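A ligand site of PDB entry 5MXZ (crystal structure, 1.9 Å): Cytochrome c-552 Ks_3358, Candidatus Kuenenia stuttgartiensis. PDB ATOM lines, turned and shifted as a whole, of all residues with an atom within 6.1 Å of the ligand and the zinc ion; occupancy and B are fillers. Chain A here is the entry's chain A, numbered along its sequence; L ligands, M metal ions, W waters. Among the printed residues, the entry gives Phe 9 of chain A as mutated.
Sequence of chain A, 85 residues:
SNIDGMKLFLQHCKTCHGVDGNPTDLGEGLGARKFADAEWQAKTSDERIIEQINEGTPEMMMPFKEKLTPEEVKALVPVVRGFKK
NE2 of Gln 52 sits close to SD of Met 61, at 3.6 Å.
The side-chain hydroxyl (OG1) of Thr 57 is in hydrogen-bond range of the side-chain amide nitrogen (NE2) of Gln 52 (2.8 Å).
NH1 of Arg 48 is in hydrogen-bond range of OE1 of Gln 52.
The backbone carbonyl oxygen (O) of Trp 40 lies within hydrogen-bond range of the side-chain hydroxyl (OG1) of Thr 44, at 2.7 Å.
The backbone NH (N) of Ala 32 sits at hydrogen-bond distance from the backbone carbonyl oxygen (O) of Gly 27 (3.0 Å).
The backbone NH (N) of Phe 64 lies within hydrogen-bond range of the backbone carbonyl oxygen (O) of Ile 53, at 2.8 Å.
Water W4 lies within hydrogen-bond range of OE1 of Gln 52 (2.6 Å), OG1 of Thr 57 (3.3 Å) and NH1 of Arg 48 (3.3 Å).
Water W6 lies within hydrogen-bond range of O2 of the ligand (2.7 Å) and OG1 of Thr 44 (2.9 Å).
Merely in contact with the zinc ion: Thr 57 (3.8 Å).
Of the 30 residues printed, 1 comes within 4 Å of the zinc ion.
The nearest printed residue that does not touch the zinc ion is Gln 52 (4.02 Å).
Merely in contact with the ligand: His 12 (3.4 Å), Thr 15 (3.9 Å), Gly 27 (3.96 Å), Leu 30 (3.4 Å), Gly 31 (3.6 Å), Ala 32 (3.4 Å), Phe 35 (3.5 Å), Ile 49 (3.9 Å), Gln 52 (3.4 Å), Ile 53 (3.6 Å), Met 60 (3.5 Å), Met 62 (3.6 Å), Phe 64 (3.5 Å), Leu 76 (3.8 Å) and Val 80 (3.9 Å).
Hydrophobic or aromatic side chains that line the ligand: His 12, His 17, Leu 30, Ala 32, Phe 35, Trp 40, Ile 49, Ile 53, Met 60, Met 61, Met 62, Phe 64, Leu 76 and Val 80.
22 residues have an atom within 4 Å of the ligand: His 12, Cys 13, Thr 15, Cys 16, His 17, Gly 27, Leu 30, Gly 31, Ala 32, Phe 35, Trp 40, Arg 48, Ile 49, Gln 52, Ile 53, Thr 57, Met 60, Met 61, Met 62, Phe 64, Leu 76 and Val 80.
The zinc ion is bound by water W5 (2.0 Å), water W4 (2.1 Å) and O3 of the ligand (2.2 Å).
The zinc ion has three donor atoms within binding distance.
A carbon (C18) of the ligand is bonded to the side-chain sulfur (SG) of Cys 13 (1.8 Å).
The side-chain sulfur (SG) of Cys 16 is covalently linked to a carbon (C25) of the ligand, at 1.8 Å.
NE2 of His 17 binds FE1 of the ligand (2.1 Å).
The side-chain sulfur (SD) of Met 61 is bound to an iron atom (FE1) of the ligand (2.2 Å).
An oxygen (O3) of the ligand lies close to the side-chain hydroxyl of Thr 57 (2.7 Å).
NH1 of Arg 48 lies within salt-bridge range of O2 of the ligand (2.9 Å).
NE1 of Trp 40 is in hydrogen-bond range of O1 of the ligand, at 3.0 Å.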
ATOM      1  N   LEU A   8     -15.336  -2.848 -28.174  1.00  0.00           N
ATOM      2  CA  LEU A   8     -16.236  -2.575 -27.042  1.00  0.00           C
ATOM      3  C   LEU A   8     -17.547  -3.336 -27.161  1.00  0.00           C
ATOM      4  O   LEU A   8     -18.054  -3.856 -26.165  1.00  0.00           O
ATOM      5  CB  LEU A   8     -16.505  -1.064 -26.915  1.00  0.00           C
ATOM      6  CG  LEU A   8     -15.365  -0.140 -26.510  1.00  0.00           C
ATOM      7  CD1 LEU A   8     -15.779   1.298 -26.786  1.00  0.00           C
ATOM      8  CD2 LEU A   8     -14.962  -0.322 -25.051  1.00  0.00           C
ATOM      9  N   PHE A   9     -18.095  -3.411 -28.373  1.00  0.00           N
ATOM     10  CA  PHE A   9     -19.349  -4.106 -28.633  1.00  0.00           C
ATOM     11  C   PHE A   9     -19.229  -5.608 -28.380  1.00  0.00           C
ATOM     12  O   PHE A   9     -20.122  -6.210 -27.784  1.00  0.00           O
ATOM     13  CB  PHE A   9     -19.834  -3.858 -30.064  1.00  0.00           C
ATOM     14  CG  PHE A   9     -21.242  -4.319 -30.321  1.00  0.00           C
ATOM     15  CD1 PHE A   9     -22.336  -3.473 -30.085  1.00  0.00           C
ATOM     16  CD2 PHE A   9     -21.492  -5.602 -30.820  1.00  0.00           C
ATOM     17  CE1 PHE A   9     -23.636  -3.888 -30.333  1.00  0.00           C
ATOM     18  CE2 PHE A   9     -22.800  -6.031 -31.049  1.00  0.00           C
ATOM     19  CZ  PHE A   9     -23.867  -5.170 -30.811  1.00  0.00           C
ATOM     20  N   HIS A  12     -18.950  -6.051 -24.505  1.00  0.00           N
ATOM     21  CA  HIS A  12     -20.019  -5.589 -23.613  1.00  0.00           C
ATOM     22  C   HIS A  12     -21.461  -5.809 -24.079  1.00  0.00           C
ATOM     23  O   HIS A  12     -22.382  -5.764 -23.265  1.00  0.00           O
ATOM     24  CB  HIS A  12     -19.836  -4.099 -23.298  1.00  0.00           C
ATOM     25  CG  HIS A  12     -18.554  -3.777 -22.586  1.00  0.00           C
ATOM     26  ND1 HIS A  12     -18.352  -4.055 -21.260  1.00  0.00           N
ATOM     27  CD2 HIS A  12     -17.410  -3.215 -23.040  1.00  0.00           C
ATOM     28  CE1 HIS A  12     -17.138  -3.661 -20.904  1.00  0.00           C
ATOM     29  NE2 HIS A  12     -16.547  -3.145 -21.975  1.00  0.00           N
ATOM     30  N   CYS A  13     -21.658  -6.045 -25.374  1.00  0.00           N
ATOM     31  CA  CYS A  13     -23.013  -5.975 -25.961  1.00  0.00           C
ATOM     32  C   CYS A  13     -23.440  -7.227 -26.715  1.00  0.00           C
ATOM     33  O   CYS A  13     -24.629  -7.542 -26.779  1.00  0.00           O
ATOM     34  CB  CYS A  13     -23.122  -4.768 -26.904  1.00  0.00           C
ATOM     35  SG  CYS A  13     -22.240  -3.267 -26.399  1.00  0.00           S
ATOM     36  N   LYS A  14     -22.461  -7.926 -27.284  1.00  0.00           N
ATOM     37  CA  LYS A  14     -22.627  -9.110 -28.133  1.00  0.00           C
ATOM     38  C   LYS A  14     -23.469 -10.231 -27.503  1.00  0.00           C
ATOM     39  O   LYS A  14     -24.206 -10.931 -28.223  1.00  0.00           O
ATOM     40  CB  LYS A  14     -21.237  -9.621 -28.573  1.00  0.00           C
ATOM     41  CG  LYS A  14     -21.159 -10.982 -29.227  1.00  0.00           C
ATOM     42  CD  LYS A  14     -19.725 -11.492 -29.230  1.00  0.00           C
ATOM     43  CE  LYS A  14     -19.627 -12.939 -28.766  1.00  0.00           C
ATOM     44  NZ  LYS A  14     -20.387 -13.907 -29.611  1.00  0.00           N
ATOM     45  N   THR A  15     -23.395 -10.365 -26.176  1.00  0.00           N
ATOM     46  CA  THR A  15     -24.124 -11.417 -25.452  1.00  0.00           C
ATOM     47  C   THR A  15     -25.647 -11.276 -25.563  1.00  0.00           C
ATOM     48  O   THR A  15     -26.362 -12.277 -25.468  1.00  0.00           O
ATOM     49  CB  THR A  15     -23.653 -11.587 -23.981  1.00  0.00           C
ATOM     50  OG1 THR A  15     -24.236 -12.769 -23.428  1.00  0.00           O
ATOM     51  CG2 THR A  15     -24.014 -10.380 -23.105  1.00  0.00           C
ATOM     52  N   CYS A  16     -26.135 -10.060 -25.774  1.00  0.00           N
ATOM     53  CA  CYS A  16     -27.565  -9.824 -25.963  1.00  0.00           C
ATOM     54  C   CYS A  16     -27.933  -9.344 -27.373  1.00  0.00           C
ATOM     55  O   CYS A  16     -28.947  -9.763 -27.928  1.00  0.00           O
ATOM     56  CB  CYS A  16     -28.106  -8.832 -24.925  1.00  0.00           C
ATOM     57  SG  CYS A  16     -28.020  -9.406 -23.208  1.00  0.00           S
ATOM     58  N   HIS A  17     -27.099  -8.460 -27.923  1.00  0.00           N
ATOM     59  CA  HIS A  17     -27.252  -7.982 -29.307  1.00  0.00           C
ATOM     60  C   HIS A  17     -26.152  -8.581 -30.173  1.00  0.00           C
ATOM     61  O   HIS A  17     -24.985  -8.170 -30.092  1.00  0.00           O
ATOM     62  CB  HIS A  17     -27.131  -6.454 -29.363  1.00  0.00           C
ATOM     63  CG  HIS A  17     -27.995  -5.714 -28.379  1.00  0.00           C
ATOM     64  ND1 HIS A  17     -29.338  -5.508 -28.585  1.00  0.00           N
ATOM     65  CD2 HIS A  17     -27.689  -5.123 -27.201  1.00  0.00           C
ATOM     66  CE1 HIS A  17     -29.825  -4.818 -27.566  1.00  0.00           C
ATOM     67  NE2 HIS A  17     -28.841  -4.571 -26.711  1.00  0.00           N
ATOM     68  N   LEU A  26     -30.718 -14.965 -25.472  1.00  0.00           N
ATOM     69  CA  LEU A  26     -30.767 -14.225 -24.204  1.00  0.00           C
ATOM     70  C   LEU A  26     -31.332 -12.820 -24.398  1.00  0.00           C
ATOM     71  O   LEU A  26     -32.265 -12.426 -23.689  1.00  0.00           O
ATOM     72  CB  LEU A  26     -29.367 -14.165 -23.558  1.00  0.00           C
ATOM     73  CG  LEU A  26     -29.135 -13.301 -22.309  1.00  0.00           C
ATOM     74  CD1 LEU A  26     -29.897 -13.821 -21.086  1.00  0.00           C
ATOM     75  CD2 LEU A  26     -27.654 -13.190 -21.997  1.00  0.00           C
ATOM     76  N   GLY A  27     -30.775 -12.076 -25.355  1.00  0.00           N
ATOM     77  CA  GLY A  27     -31.243 -10.717 -25.673  1.00  0.00           C
ATOM     78  C   GLY A  27     -32.735 -10.613 -25.904  1.00  0.00           C
ATOM     79  O   GLY A  27     -33.412  -9.791 -25.283  1.00  0.00           O
ATOM     80  N   LEU A  30     -34.970 -11.170 -22.866  1.00  0.00           N
ATOM     81  CA  LEU A  30     -35.013  -9.993 -21.998  1.00  0.00           C
ATOM     82  C   LEU A  30     -35.806  -8.826 -22.601  1.00  0.00           C
ATOM     83  O   LEU A  30     -36.223  -7.919 -21.875  1.00  0.00           O
ATOM     84  CB  LEU A  30     -33.587  -9.548 -21.627  1.00  0.00           C
ATOM     85  CG  LEU A  30     -32.799 -10.533 -20.746  1.00  0.00           C
ATOM     86  CD1 LEU A  30     -31.314 -10.288 -20.927  1.00  0.00           C
ATOM     87  CD2 LEU A  30     -33.200 -10.465 -19.283  1.00  0.00           C
ATOM     88  N   GLY A  31     -36.019  -8.865 -23.920  1.00  0.00           N
ATOM     89  CA  GLY A  31     -36.881  -7.905 -24.596  1.00  0.00           C
ATOM     90  C   GLY A  31     -36.250  -7.080 -25.702  1.00  0.00           C
ATOM     91  O   GLY A  31     -36.868  -6.123 -26.190  1.00  0.00           O
ATOM     92  N   ALA A  32     -35.032  -7.455 -26.115  1.00  0.00           N
ATOM     93  CA  ALA A  32     -34.340  -6.742 -27.187  1.00  0.00           C
ATOM     94  C   ALA A  32     -34.923  -7.073 -28.561  1.00  0.00           C
ATOM     95  O   ALA A  32     -35.428  -8.178 -28.773  1.00  0.00           O
ATOM     96  CB  ALA A  32     -32.844  -7.037 -27.162  1.00  0.00           C
ATOM     97  N   ARG A  33     -34.869  -6.106 -29.475  1.00  0.00           N
ATOM     98  CA  ARG A  33     -35.277  -6.271 -30.863  1.00  0.00           C
ATOM     99  C   ARG A  33     -34.078  -6.099 -31.806  1.00  0.00           C
ATOM    100  O   ARG A  33     -32.951  -5.877 -31.355  1.00  0.00           O
ATOM    101  CB  ARG A  33     -36.399  -5.276 -31.228  1.00  0.00           C
ATOM    102  CG  ARG A  33     -37.746  -5.557 -30.583  1.00  0.00           C
ATOM    103  CD  ARG A  33     -37.932  -4.738 -29.321  1.00  0.00           C
ATOM    104  NE  ARG A  33     -39.306  -4.692 -28.845  1.00  0.00           N
ATOM    105  CZ  ARG A  33     -40.135  -3.661 -28.985  1.00  0.00           C
ATOM    106  NH1 ARG A  33     -39.745  -2.537 -29.593  1.00  0.00           N
ATOM    107  NH2 ARG A  33     -41.357  -3.745 -28.495  1.00  0.00           N
ATOM    108  N   PHE A  35     -31.387  -4.555 -34.376  1.00  0.00           N
ATOM    109  CA  PHE A  35     -30.782  -3.305 -34.844  1.00  0.00           C
ATOM    110  C   PHE A  35     -30.886  -3.174 -36.362  1.00  0.00           C
ATOM    111  O   PHE A  35     -31.053  -2.074 -36.890  1.00  0.00           O
ATOM    112  CB  PHE A  35     -29.311  -3.178 -34.423  1.00  0.00           C
ATOM    113  CG  PHE A  35     -29.101  -2.963 -32.950  1.00  0.00           C
ATOM    114  CD1 PHE A  35     -30.026  -2.283 -32.163  1.00  0.00           C
ATOM    115  CD2 PHE A  35     -27.928  -3.437 -32.350  1.00  0.00           C
ATOM    116  CE1 PHE A  35     -29.810  -2.096 -30.794  1.00  0.00           C
ATOM    117  CE2 PHE A  35     -27.702  -3.243 -30.992  1.00  0.00           C
ATOM    118  CZ  PHE A  35     -28.635  -2.580 -30.216  1.00  0.00           C
ATOM    119  N   TRP A  40     -36.456   1.162 -37.554  1.00  0.00           N
ATOM    120  CA  TRP A  40     -35.903   1.416 -36.216  1.00  0.00           C
ATOM    121  C   TRP A  40     -34.769   2.431 -36.282  1.00  0.00           C
ATOM    122  O   TRP A  40     -34.750   3.388 -35.505  1.00  0.00           O
ATOM    123  CB  TRP A  40     -35.448   0.137 -35.498  1.00  0.00           C
ATOM    124  CG  TRP A  40     -34.915   0.473 -34.114  1.00  0.00           C
ATOM    125  CD1 TRP A  40     -35.657   0.676 -32.977  1.00  0.00           C
ATOM    126  CD2 TRP A  40     -33.549   0.691 -33.742  1.00  0.00           C
ATOM    127  NE1 TRP A  40     -34.842   0.992 -31.925  1.00  0.00           N
ATOM    128  CE2 TRP A  40     -33.539   1.012 -32.363  1.00  0.00           C
ATOM    129  CE3 TRP A  40     -32.330   0.652 -34.434  1.00  0.00           C
ATOM    130  CZ2 TRP A  40     -32.351   1.290 -31.665  1.00  0.00           C
ATOM    131  CZ3 TRP A  40     -31.150   0.924 -33.738  1.00  0.00           C
ATOM    132  CH2 TRP A  40     -31.177   1.241 -32.361  1.00  0.00           C
ATOM    133  N   THR A  44     -34.761   6.324 -34.623  1.00  0.00           N
ATOM    134  CA  THR A  44     -33.958   6.374 -33.407  1.00  0.00           C
ATOM    135  C   THR A  44     -32.804   7.349 -33.551  1.00  0.00           C
ATOM    136  O   THR A  44     -31.995   7.240 -34.480  1.00  0.00           O
ATOM    137  CB  THR A  44     -33.448   4.968 -33.008  1.00  0.00           C
ATOM    138  OG1 THR A  44     -34.552   4.061 -32.947  1.00  0.00           O
ATOM    139  CG2 THR A  44     -32.732   4.989 -31.663  1.00  0.00           C
ATOM    140  N   ARG A  48     -30.819   8.942 -28.150  1.00  0.00           N
ATOM    141  CA  ARG A  48     -31.582   7.799 -27.618  1.00  0.00           C
ATOM    142  C   ARG A  48     -30.673   6.583 -27.429  1.00  0.00           C
ATOM    143  O   ARG A  48     -30.727   5.922 -26.379  1.00  0.00           O
ATOM    144  CB  ARG A  48     -32.793   7.478 -28.502  1.00  0.00           C
ATOM    145  CG  ARG A  48     -33.585   6.221 -28.156  1.00  0.00           C
ATOM    146  CD  ARG A  48     -34.600   6.399 -27.003  1.00  0.00           C
ATOM    147  NE  ARG A  48     -33.967   6.459 -25.676  1.00  0.00           N
ATOM    148  CZ  ARG A  48     -33.603   5.402 -24.948  1.00  0.00           C
ATOM    149  NH1 ARG A  48     -33.773   4.159 -25.378  1.00  0.00           N
ATOM    150  NH2 ARG A  48     -33.040   5.596 -23.767  1.00  0.00           N
ATOM    151  N   ILE A  49     -29.841   6.306 -28.433  1.00  0.00           N
ATOM    152  CA  ILE A  49     -28.863   5.214 -28.369  1.00  0.00           C
ATOM    153  C   ILE A  49     -27.892   5.418 -27.199  1.00  0.00           C
ATOM    154  O   ILE A  49     -27.693   4.502 -26.391  1.00  0.00           O
ATOM    155  CB  ILE A  49     -28.123   5.019 -29.726  1.00  0.00           C
ATOM    156  CG1 ILE A  49     -29.101   4.548 -30.827  1.00  0.00           C
ATOM    157  CG2 ILE A  49     -26.962   4.036 -29.592  1.00  0.00           C
ATOM    158  CD1 ILE A  49     -28.619   4.719 -32.263  1.00  0.00           C
ATOM    159  N   GLN A  52     -29.601   5.054 -23.817  1.00  0.00           N
ATOM    160  CA  GLN A  52     -29.846   3.623 -23.572  1.00  0.00           C
ATOM    161  C   GLN A  52     -28.601   2.900 -23.063  1.00  0.00           C
ATOM    162  O   GLN A  52     -28.698   2.125 -22.114  1.00  0.00           O
ATOM    163  CB  GLN A  52     -30.414   2.931 -24.812  1.00  0.00           C
ATOM    164  CG  GLN A  52     -30.795   1.480 -24.560  1.00  0.00           C
ATOM    165  CD  GLN A  52     -31.970   1.310 -23.611  1.00  0.00           C
ATOM    166  OE1 GLN A  52     -32.920   2.105 -23.627  1.00  0.00           O
ATOM    167  NE2 GLN A  52     -31.912   0.278 -22.776  1.00  0.00           N
ATOM    168  N   ILE A  53     -27.451   3.147 -23.689  1.00  0.00           N
ATOM    169  CA  ILE A  53     -26.184   2.558 -23.229  1.00  0.00           C
ATOM    170  C   ILE A  53     -25.856   3.068 -21.817  1.00  0.00           C
ATOM    171  O   ILE A  53     -25.533   2.277 -20.930  1.00  0.00           O
ATOM    172  CB  ILE A  53     -25.008   2.846 -24.204  1.00  0.00           C
ATOM    173  CG1 ILE A  53     -25.351   2.351 -25.611  1.00  0.00           C
ATOM    174  CG2 ILE A  53     -23.698   2.213 -23.715  1.00  0.00           C
ATOM    175  CD1 ILE A  53     -24.530   2.970 -26.738  1.00  0.00           C
ATOM    176  N   GLY A  56     -29.511   2.125 -19.451  1.00  0.00           N
ATOM    177  CA  GLY A  56     -30.166   0.825 -19.602  1.00  0.00           C
ATOM    178  C   GLY A  56     -31.665   0.922 -19.424  1.00  0.00           C
ATOM    179  O   GLY A  56     -32.263   1.985 -19.597  1.00  0.00           O
ATOM    180  N   THR A  57     -32.266  -0.221 -19.085  1.00  0.00           N
ATOM    181  CA  THR A  57     -33.694  -0.354 -18.836  1.00  0.00           C
ATOM    182  C   THR A  57     -33.828  -1.377 -17.699  1.00  0.00           C
ATOM    183  O   THR A  57     -33.320  -2.490 -17.825  1.00  0.00           O
ATOM    184  CB  THR A  57     -34.453  -0.844 -20.086  1.00  0.00           C
ATOM    185  OG1 THR A  57     -34.239   0.069 -21.169  1.00  0.00           O
ATOM    186  CG2 THR A  57     -35.966  -0.980 -19.823  1.00  0.00           C
ATOM    187  N   MET A  60     -34.035  -5.337 -17.890  1.00  0.00           N
ATOM    188  CA  MET A  60     -33.811  -5.660 -19.304  1.00  0.00           C
ATOM    189  C   MET A  60     -32.354  -5.491 -19.733  1.00  0.00           C
ATOM    190  O   MET A  60     -31.744  -6.424 -20.271  1.00  0.00           O
ATOM    191  CB  MET A  60     -34.732  -4.817 -20.195  1.00  0.00           C
ATOM    192  CG  MET A  60     -36.224  -5.064 -19.987  1.00  0.00           C
ATOM    193  SD  MET A  60     -37.185  -4.372 -21.341  1.00  0.00           S
ATOM    194  CE  MET A  60     -38.805  -4.321 -20.598  1.00  0.00           C
ATOM    195  N   MET A  61     -31.806  -4.296 -19.480  1.00  0.00           N
ATOM    196  CA  MET A  61     -30.448  -3.953 -19.868  1.00  0.00           C
ATOM    197  C   MET A  61     -29.796  -3.159 -18.737  1.00  0.00           C
ATOM    198  O   MET A  61     -30.380  -2.192 -18.247  1.00  0.00           O
ATOM    199  CB  MET A  61     -30.468  -3.128 -21.173  1.00  0.00           C
ATOM    200  CG  MET A  61     -29.093  -2.796 -21.748  1.00  0.00           C
ATOM    201  SD  MET A  61     -29.179  -1.983 -23.357  1.00  0.00           S
ATOM    202  CE  MET A  61     -27.797  -0.864 -23.166  1.00  0.00           C
ATOM    203  N   MET A  62     -28.598  -3.590 -18.324  1.00  0.00           N
ATOM    204  CA  MET A  62     -27.822  -2.874 -17.314  1.00  0.00           C
ATOM    205  C   MET A  62     -27.364  -1.504 -17.831  1.00  0.00           C
ATOM    206  O   MET A  62     -27.197  -1.327 -19.041  1.00  0.00           O
ATOM    207  CB  MET A  62     -26.635  -3.720 -16.801  1.00  0.00           C
ATOM    208  CG  MET A  62     -25.544  -4.060 -17.831  1.00  0.00           C
ATOM    209  SD  MET A  62     -26.030  -5.327 -19.027  1.00  0.00           S
ATOM    210  CE  MET A  62     -25.843  -6.830 -18.067  1.00  0.00           C
ATOM    211  N   PHE A  64     -24.500   1.252 -18.537  1.00  0.00           N
ATOM    212  CA  PHE A  64     -23.060   1.167 -18.817  1.00  0.00           C
ATOM    213  C   PHE A  64     -22.265   2.424 -18.473  1.00  0.00           C
ATOM    214  O   PHE A  64     -21.047   2.450 -18.676  1.00  0.00           O
ATOM    215  CB  PHE A  64     -22.814   0.744 -20.278  1.00  0.00           C
ATOM    216  CG  PHE A  64     -23.107  -0.703 -20.545  1.00  0.00           C
ATOM    217  CD1 PHE A  64     -24.395  -1.132 -20.835  1.00  0.00           C
ATOM    218  CD2 PHE A  64     -22.079  -1.642 -20.499  1.00  0.00           C
ATOM    219  CE1 PHE A  64     -24.656  -2.483 -21.078  1.00  0.00           C
ATOM    220  CE2 PHE A  64     -22.338  -3.000 -20.735  1.00  0.00           C
ATOM    221  CZ  PHE A  64     -23.627  -3.411 -21.024  1.00  0.00           C
ATOM    222  N   LEU A  68     -18.276   2.671 -18.885  1.00  0.00           N
ATOM    223  CA  LEU A  68     -17.779   3.291 -20.117  1.00  0.00           C
ATOM    224  C   LEU A  68     -17.800   4.802 -20.028  1.00  0.00           C
ATOM    225  O   LEU A  68     -18.717   5.379 -19.446  1.00  0.00           O
ATOM    226  CB  LEU A  68     -18.599   2.827 -21.337  1.00  0.00           C
ATOM    227  CG  LEU A  68     -18.725   1.331 -21.638  1.00  0.00           C
ATOM    228  CD1 LEU A  68     -19.736   1.102 -22.748  1.00  0.00           C
ATOM    229  CD2 LEU A  68     -17.392   0.680 -21.994  1.00  0.00           C
ATOM    230  N   LEU A  76     -19.705   3.520 -29.780  1.00  0.00           N
ATOM    231  CA  LEU A  76     -20.648   2.403 -30.011  1.00  0.00           C
ATOM    232  C   LEU A  76     -21.782   2.758 -30.985  1.00  0.00           C
ATOM    233  O   LEU A  76     -22.404   1.852 -31.540  1.00  0.00           O
ATOM    234  CB  LEU A  76     -21.214   1.887 -28.685  1.00  0.00           C
ATOM    235  CG  LEU A  76     -20.298   1.015 -27.827  1.00  0.00           C
ATOM    236  CD1 LEU A  76     -20.791   0.994 -26.388  1.00  0.00           C
ATOM    237  CD2 LEU A  76     -20.176  -0.405 -28.373  1.00  0.00           C
ATOM    238  N   VAL A  80     -23.883   0.198 -33.605  1.00  0.00           N
ATOM    239  CA  VAL A  80     -25.338   0.021 -33.528  1.00  0.00           C
ATOM    240  C   VAL A  80     -25.996   0.355 -34.879  1.00  0.00           C
ATOM    241  O   VAL A  80     -26.903  -0.360 -35.337  1.00  0.00           O
ATOM    242  CB  VAL A  80     -25.956   0.870 -32.376  1.00  0.00           C
ATOM    243  CG1 VAL A  80     -27.483   0.926 -32.458  1.00  0.00           C
ATOM    244  CG2 VAL A  80     -25.520   0.330 -31.012  1.00  0.00           C
HETATM  245 FE1  LIG L   1     -28.936  -3.288 -25.063  1.00  0.00          FE
HETATM  246  C1  LIG L   1     -32.072  -2.047 -25.753  1.00  0.00           C
HETATM  247  C2  LIG L   1     -27.521  -1.009 -27.219  1.00  0.00           C
HETATM  248  C3  LIG L   1     -25.815  -4.169 -23.884  1.00  0.00           C
HETATM  249  C4  LIG L   1     -30.321  -6.030 -23.577  1.00  0.00           C
HETATM  250  N1  LIG L   1     -29.680  -1.749 -26.266  1.00  0.00           N
HETATM  251  C5  LIG L   1     -30.962  -1.431 -26.497  1.00  0.00           C
HETATM  252  C6  LIG L   1     -31.184  -0.329 -27.442  1.00  0.00           C
HETATM  253  C7  LIG L   1     -29.827   0.006 -27.890  1.00  0.00           C
HETATM  254  C8  LIG L   1     -28.992  -0.952 -27.097  1.00  0.00           C
HETATM  255  C9  LIG L   1     -29.397   1.058 -28.875  1.00  0.00           C
HETATM  256  C10 LIG L   1     -32.513   0.240 -27.869  1.00  0.00           C
HETATM  257  C11 LIG L   1     -32.890   1.621 -27.407  1.00  0.00           C
HETATM  258  C12 LIG L   1     -34.154   1.996 -28.171  1.00  0.00           C
HETATM  259  O1  LIG L   1     -34.689   1.189 -28.958  1.00  0.00           O
HETATM  260  O2  LIG L   1     -34.607   3.136 -27.991  1.00  0.00           O
HETATM  261  N2  LIG L   1     -26.981  -2.666 -25.463  1.00  0.00           N
HETATM  262  C13 LIG L   1     -26.568  -1.759 -26.385  1.00  0.00           C
HETATM  263  C14 LIG L   1     -25.099  -1.533 -26.469  1.00  0.00           C
HETATM  264  C15 LIG L   1     -24.633  -2.485 -25.455  1.00  0.00           C
HETATM  265  C16 LIG L   1     -25.839  -3.145 -24.923  1.00  0.00           C
HETATM  266  C17 LIG L   1     -24.329  -0.600 -27.369  1.00  0.00           C
HETATM  267  C18 LIG L   1     -23.253  -2.740 -25.025  1.00  0.00           C
HETATM  268  C19 LIG L   1     -22.569  -1.618 -24.282  1.00  0.00           C
HETATM  269  N3  LIG L   1     -28.183  -4.841 -23.889  1.00  0.00           N
HETATM  270  C20 LIG L   1     -26.903  -5.102 -23.558  1.00  0.00           C
HETATM  271  C21 LIG L   1     -26.686  -6.347 -22.752  1.00  0.00           C
HETATM  272  C22 LIG L   1     -28.061  -6.866 -22.669  1.00  0.00           C
HETATM  273  C23 LIG L   1     -28.878  -5.897 -23.420  1.00  0.00           C
HETATM  274  C24 LIG L   1     -25.399  -6.888 -22.194  1.00  0.00           C
HETATM  275  C25 LIG L   1     -28.518  -8.134 -22.017  1.00  0.00           C
HETATM  276  C26 LIG L   1     -28.301  -8.314 -20.540  1.00  0.00           C
HETATM  277  N4  LIG L   1     -30.891  -3.914 -24.693  1.00  0.00           N
HETATM  278  C27 LIG L   1     -31.281  -5.039 -24.085  1.00  0.00           C
HETATM  279  C28 LIG L   1     -32.746  -5.209 -23.958  1.00  0.00           C
HETATM  280  C29 LIG L   1     -33.266  -4.015 -24.627  1.00  0.00           C
HETATM  281  C30 LIG L   1     -32.030  -3.312 -25.031  1.00  0.00           C
HETATM  282  C31 LIG L   1     -33.519  -6.346 -23.326  1.00  0.00           C
HETATM  283  C32 LIG L   1     -34.687  -3.557 -24.816  1.00  0.00           C
HETATM  284  C33 LIG L   1     -34.904  -2.498 -23.726  1.00  0.00           C
HETATM  285  C34 LIG L   1     -35.415  -1.152 -24.211  1.00  0.00           C
HETATM  286  O3  LIG L   1     -35.796  -0.318 -23.357  1.00  0.00           O
HETATM  287  O4  LIG L   1     -35.455  -0.881 -25.429  1.00  0.00           O
HETATM  288 ZN    ZN M   1     -36.898   1.567 -23.384  1.00  0.00          ZN
HETATM  289  O   HOH W   1     -22.247  -7.416 -20.933  1.00  0.00           O
HETATM  290  O   HOH W   2     -35.480  -1.427 -28.055  1.00  0.00           O
HETATM  291  O   HOH W   3     -37.222   3.129 -27.298  1.00  0.00           O
HETATM  292  O   HOH W   4     -35.293   2.697 -22.776  1.00  0.00           O
HETATM  293  O   HOH W   5     -36.735   1.490 -25.350  1.00  0.00           O
HETATM  294  O   HOH W   6     -35.675   4.030 -30.302  1.00  0.00           O
